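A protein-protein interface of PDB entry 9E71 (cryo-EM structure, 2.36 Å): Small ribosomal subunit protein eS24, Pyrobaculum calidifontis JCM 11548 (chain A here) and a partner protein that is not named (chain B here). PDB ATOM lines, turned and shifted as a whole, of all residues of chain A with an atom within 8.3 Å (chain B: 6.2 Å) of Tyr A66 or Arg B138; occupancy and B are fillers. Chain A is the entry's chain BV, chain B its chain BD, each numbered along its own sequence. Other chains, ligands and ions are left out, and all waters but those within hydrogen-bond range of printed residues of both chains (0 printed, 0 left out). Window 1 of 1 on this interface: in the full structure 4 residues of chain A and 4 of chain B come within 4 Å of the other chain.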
ATOM      1  N   LYS A  63       6.996   6.632 -17.998  1.00  0.00           N
ATOM      2  CA  LYS A  63       6.986   5.177 -18.088  1.00  0.00           C
ATOM      3  C   LYS A  63       8.112   4.735 -19.012  1.00  0.00           C
ATOM      4  O   LYS A  63       8.178   5.169 -20.166  1.00  0.00           O
ATOM      5  CB  LYS A  63       5.622   4.687 -18.586  1.00  0.00           C
ATOM      6  CG  LYS A  63       5.559   3.257 -19.113  1.00  0.00           C
ATOM      7  CD  LYS A  63       6.160   2.230 -18.166  1.00  0.00           C
ATOM      8  CE  LYS A  63       6.572   0.985 -18.937  1.00  0.00           C
ATOM      9  NZ  LYS A  63       7.497   0.106 -18.166  1.00  0.00           N
ATOM     10  N   THR A  64       8.978   3.862 -18.504  1.00  0.00           N
ATOM     11  CA  THR A  64      10.172   3.415 -19.209  1.00  0.00           C
ATOM     12  C   THR A  64       9.988   1.999 -19.730  1.00  0.00           C
ATOM     13  O   THR A  64       9.561   1.107 -18.995  1.00  0.00           O
ATOM     14  CB  THR A  64      11.394   3.460 -18.294  1.00  0.00           C
ATOM     15  OG1 THR A  64      11.429   4.710 -17.600  1.00  0.00           O
ATOM     16  CG2 THR A  64      12.665   3.300 -19.101  1.00  0.00           C
ATOM     17  N   GLU A  65      10.349   1.796 -20.992  1.00  0.00           N
ATOM     18  CA  GLU A  65      10.183   0.504 -21.641  1.00  0.00           C
ATOM     19  C   GLU A  65      11.058  -0.560 -20.992  1.00  0.00           C
ATOM     20  O   GLU A  65      12.058  -0.263 -20.336  1.00  0.00           O
ATOM     21  CB  GLU A  65      10.531   0.605 -23.120  1.00  0.00           C
ATOM     22  CG  GLU A  65       9.567   1.424 -23.929  1.00  0.00           C
ATOM     23  CD  GLU A  65       9.676   1.133 -25.405  1.00  0.00           C
ATOM     24  OE1 GLU A  65      10.554   0.333 -25.789  1.00  0.00           O
ATOM     25  OE2 GLU A  65       8.885   1.701 -26.185  1.00  0.00           O
ATOM     26  N   TYR A  66      10.661  -1.815 -21.179  1.00  0.00           N
ATOM     27  CA  TYR A  66      11.486  -2.932 -20.745  1.00  0.00           C
ATOM     28  C   TYR A  66      12.665  -3.108 -21.693  1.00  0.00           C
ATOM     29  O   TYR A  66      12.510  -3.043 -22.915  1.00  0.00           O
ATOM     30  CB  TYR A  66      10.655  -4.214 -20.691  1.00  0.00           C
ATOM     31  CG  TYR A  66      11.416  -5.421 -20.192  1.00  0.00           C
ATOM     32  CD1 TYR A  66      11.569  -5.652 -18.836  1.00  0.00           C
ATOM     33  CD2 TYR A  66      11.985  -6.326 -21.078  1.00  0.00           C
ATOM     34  CE1 TYR A  66      12.264  -6.744 -18.375  1.00  0.00           C
ATOM     35  CE2 TYR A  66      12.683  -7.420 -20.626  1.00  0.00           C
ATOM     36  CZ  TYR A  66      12.818  -7.626 -19.274  1.00  0.00           C
ATOM     37  OH  TYR A  66      13.511  -8.717 -18.814  1.00  0.00           O
ATOM     38  N   GLY A  67      13.849  -3.323 -21.129  1.00  0.00           N
ATOM     39  CA  GLY A  67      14.991  -3.732 -21.917  1.00  0.00           C
ATOM     40  C   GLY A  67      15.644  -2.661 -22.755  1.00  0.00           C
ATOM     41  O   GLY A  67      16.523  -2.984 -23.559  1.00  0.00           O
ATOM     42  N   ILE A  68      15.255  -1.398 -22.598  1.00  0.00           N
ATOM     43  CA  ILE A  68      15.835  -0.323 -23.391  1.00  0.00           C
ATOM     44  C   ILE A  68      15.604   0.984 -22.653  1.00  0.00           C
ATOM     45  O   ILE A  68      14.585   1.162 -21.982  1.00  0.00           O
ATOM     46  CB  ILE A  68      15.232  -0.294 -24.819  1.00  0.00           C
ATOM     47  CG1 ILE A  68      15.900   0.791 -25.662  1.00  0.00           C
ATOM     48  CG2 ILE A  68      13.736  -0.067 -24.760  1.00  0.00           C
ATOM     49  CD1 ILE A  68      16.266   0.343 -27.053  1.00  0.00           C
ATOM     50  N   GLY A  69      16.557   1.902 -22.778  1.00  0.00           N
ATOM     51  CA  GLY A  69      16.448   3.199 -22.147  1.00  0.00           C
ATOM     52  C   GLY A  69      15.588   4.177 -22.918  1.00  0.00           C
ATOM     53  O   GLY A  69      16.071   5.220 -23.365  1.00  0.00           O
ATOM     54  N   LYS A  70      14.310   3.854 -23.084  1.00  0.00           N
ATOM     55  CA  LYS A  70      13.342   4.746 -23.704  1.00  0.00           C
ATOM     56  C   LYS A  70      12.209   4.996 -22.722  1.00  0.00           C
ATOM     57  O   LYS A  70      11.773   4.079 -22.024  1.00  0.00           O
ATOM     58  CB  LYS A  70      12.796   4.154 -25.003  1.00  0.00           C
ATOM     59  CG  LYS A  70      12.883   5.091 -26.189  1.00  0.00           C
ATOM     60  CD  LYS A  70      11.948   4.664 -27.307  1.00  0.00           C
ATOM     61  CE  LYS A  70      12.373   3.336 -27.907  1.00  0.00           C
ATOM     62  NZ  LYS A  70      11.904   3.191 -29.313  1.00  0.00           N
ATOM     63  N   SER A  71      11.753   6.244 -22.644  1.00  0.00           N
ATOM     64  CA  SER A  71      10.690   6.604 -21.719  1.00  0.00           C
ATOM     65  C   SER A  71       9.701   7.532 -22.402  1.00  0.00           C
ATOM     66  O   SER A  71      10.085   8.439 -23.142  1.00  0.00           O
ATOM     67  CB  SER A  71      11.238   7.273 -20.454  1.00  0.00           C
ATOM     68  OG  SER A  71      12.396   6.610 -19.990  1.00  0.00           O
ATOM     69  N   VAL B 133      21.268 -10.238 -25.740  1.00  0.00           N
ATOM     70  CA  VAL B 133      20.641 -10.413 -27.042  1.00  0.00           C
ATOM     71  C   VAL B 133      19.640  -9.286 -27.241  1.00  0.00           C
ATOM     72  O   VAL B 133      18.710  -9.122 -26.444  1.00  0.00           O
ATOM     73  CB  VAL B 133      19.963 -11.784 -27.160  1.00  0.00           C
ATOM     74  CG1 VAL B 133      19.092 -11.829 -28.394  1.00  0.00           C
ATOM     75  CG2 VAL B 133      21.007 -12.879 -27.202  1.00  0.00           C
ATOM     76  N   LEU B 134      19.831  -8.511 -28.302  1.00  0.00           N
ATOM     77  CA  LEU B 134      18.962  -7.394 -28.636  1.00  0.00           C
ATOM     78  C   LEU B 134      18.120  -7.770 -29.841  1.00  0.00           C
ATOM     79  O   LEU B 134      18.648  -8.262 -30.842  1.00  0.00           O
ATOM     80  CB  LEU B 134      19.772  -6.133 -28.934  1.00  0.00           C
ATOM     81  CG  LEU B 134      20.630  -5.595 -27.794  1.00  0.00           C
ATOM     82  CD1 LEU B 134      21.500  -4.455 -28.280  1.00  0.00           C
ATOM     83  CD2 LEU B 134      19.757  -5.137 -26.657  1.00  0.00           C
ATOM     84  N   VAL B 135      16.814  -7.544 -29.739  1.00  0.00           N
ATOM     85  CA  VAL B 135      15.910  -7.791 -30.853  1.00  0.00           C
ATOM     86  C   VAL B 135      15.395  -6.454 -31.360  1.00  0.00           C
ATOM     87  O   VAL B 135      14.471  -5.872 -30.785  1.00  0.00           O
ATOM     88  CB  VAL B 135      14.753  -8.716 -30.446  1.00  0.00           C
ATOM     89  CG1 VAL B 135      13.677  -8.712 -31.515  1.00  0.00           C
ATOM     90  CG2 VAL B 135      15.269 -10.119 -30.210  1.00  0.00           C
ATOM     91  N   ALA B 136      16.007  -5.954 -32.434  1.00  0.00           N
ATOM     92  CA  ALA B 136      15.661  -4.666 -33.027  1.00  0.00           C
ATOM     93  C   ALA B 136      15.888  -3.507 -32.063  1.00  0.00           C
ATOM     94  O   ALA B 136      15.212  -2.482 -32.147  1.00  0.00           O
ATOM     95  CB  ALA B 136      14.217  -4.657 -33.535  1.00  0.00           C
ATOM     96  N   GLY B 137      16.837  -3.649 -31.144  1.00  0.00           N
ATOM     97  CA  GLY B 137      17.197  -2.596 -30.221  1.00  0.00           C
ATOM     98  C   GLY B 137      16.843  -2.873 -28.778  1.00  0.00           C
ATOM     99  O   GLY B 137      17.485  -2.314 -27.881  1.00  0.00           O
ATOM    100  N   ARG B 138      15.852  -3.717 -28.525  1.00  0.00           N
ATOM    101  CA  ARG B 138      15.420  -4.020 -27.172  1.00  0.00           C
ATOM    102  C   ARG B 138      15.961  -5.372 -26.730  1.00  0.00           C
ATOM    103  O   ARG B 138      16.116  -6.299 -27.526  1.00  0.00           O
ATOM    104  CB  ARG B 138      13.894  -4.010 -27.074  1.00  0.00           C
ATOM    105  CG  ARG B 138      13.367  -4.182 -25.666  1.00  0.00           C
ATOM    106  CD  ARG B 138      11.923  -4.623 -25.674  1.00  0.00           C
ATOM    107  NE  ARG B 138      11.153  -3.907 -26.680  1.00  0.00           N
ATOM    108  CZ  ARG B 138      10.733  -2.657 -26.549  1.00  0.00           C
ATOM    109  NH1 ARG B 138      10.991  -1.952 -25.462  1.00  0.00           N
ATOM    110  NH2 ARG B 138      10.038  -2.101 -27.535  1.00  0.00           N
ATOM    111  N   ARG B 139      16.254  -5.470 -25.438  1.00  0.00           N
ATOM    112  CA  ARG B 139      16.703  -6.718 -24.841  1.00  0.00           C
ATOM    113  C   ARG B 139      15.507  -7.638 -24.660  1.00  0.00           C
ATOM    114  O   ARG B 139      14.546  -7.288 -23.969  1.00  0.00           O
ATOM    115  CB  ARG B 139      17.379  -6.466 -23.496  1.00  0.00           C
ATOM    116  CG  ARG B 139      18.824  -6.048 -23.592  1.00  0.00           C
ATOM    117  CD  ARG B 139      19.371  -5.748 -22.220  1.00  0.00           C
ATOM    118  NE  ARG B 139      18.327  -5.232 -21.346  1.00  0.00           N
ATOM    119  CZ  ARG B 139      18.435  -4.126 -20.626  1.00  0.00           C
ATOM    120  NH1 ARG B 139      19.533  -3.388 -20.654  1.00  0.00           N
ATOM    121  NH2 ARG B 139      17.418  -3.750 -19.859  1.00  0.00           N
ATOM    122  N   VAL B 140      15.563  -8.806 -25.285  1.00  0.00           N
ATOM    123  CA  VAL B 140      14.583  -9.862 -25.077  1.00  0.00           C
ATOM    124  C   VAL B 140      15.275 -10.936 -24.253  1.00  0.00           C
ATOM    125  O   VAL B 140      16.204 -11.593 -24.730  1.00  0.00           O
ATOM    126  CB  VAL B 140      14.057 -10.415 -26.405  1.00  0.00           C
ATOM    127  CG1 VAL B 140      13.523 -11.814 -26.214  1.00  0.00           C
ATOM    128  CG2 VAL B 140      12.987  -9.502 -26.968  1.00  0.00           C
ATOM    129  N   THR B 141      14.841 -11.106 -23.008  1.00  0.00           N
ATOM    130  CA  THR B 141      15.536 -11.961 -22.060  1.00  0.00           C
ATOM    131  C   THR B 141      14.877 -13.320 -21.890  1.00  0.00           C
ATOM    132  O   THR B 141      15.265 -14.075 -20.994  1.00  0.00           O
ATOM    133  CB  THR B 141      15.649 -11.264 -20.704  1.00  0.00           C
ATOM    134  OG1 THR B 141      14.432 -10.567 -20.424  1.00  0.00           O
ATOM    135  CG2 THR B 141      16.806 -10.271 -20.708  1.00  0.00           C
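The guanidinium group of Arg B138 is in salt-bridge range of the side-chain carboxylate of Glu A65 (3.0 Å).
The backbone carbonyl oxygen of Tyr A66 sits close to the guanidinium group of Arg B138, 3.2 Å away.
The backbone NH (N) of Arg B139 lies within hydrogen-bond range of the backbone carbonyl oxygen (O) of Gly A67 (3.1 Å).
The side-chain hydroxyl (OH) of Tyr A66 is in hydrogen-bond range of the side-chain hydroxyl (OG1) of Thr B141, at 2.6 Å.
N of Glu A65 lies within hydrogen-bond range of O of Lys A70 (2.9 Å).
Tyr A66 touches Arg B139.
Gly A67 touches Arg B138 (O to CA, 3.9 Å).
O of Gly B137 touches CD1 of Ile A68 (3.0 Å).
Ile A68 touches Arg B138 (CG2 to NH1, 3.4 Å).
Tyr A66 touches just these residues of chain B: Arg B138, Arg B139 and Thr B141.
Of chain A, only Glu A65, Tyr A66, Gly A67 and Ile A68 come within 4 Å of Arg B138.
Printed residues of chain A within 4 Å of Gly B137: Ile A68.
Of the printed residues of chain B, Gly A67 touches Arg B138 (3.9 Å) and Arg B139 (3.1 Å).
Printed residues of chain A within 4 Å of Thr B141: Tyr A66 (2.6 Å).
Of the printed residues of chain A, Arg B139 touches Tyr A66 (3.8 Å) and Gly A67 (3.1 Å).
Printed residues of chain B within 4 Å of Glu A65: Arg B138.
Printed residues of chain B within 4 Å of Ile A68: Gly B137 and Arg B138.
Val B135 touches none of the printed residues of chain A.
The nearest residue of chain B that does not touch Tyr A66 is Val B140 (5.4 Å).
The nearest residue of chain A that does not touch Arg B138 is Lys A70 (5.9 Å).
The nearest printed residue of chain B that does not touch Gly A67 is Gly B137 (4.5 Å).
Of the 9 printed residues of chain A, 4 touch a printed residue of chain B.
Among the printed residues, 8 pairs touch across the chains.
Among the printed residues, Asp or Glu carboxylates within 4 Å of a Lys or Arg side-chain nitrogen of the other chain: Glu A65 with Arg B138 (2.3 Å).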
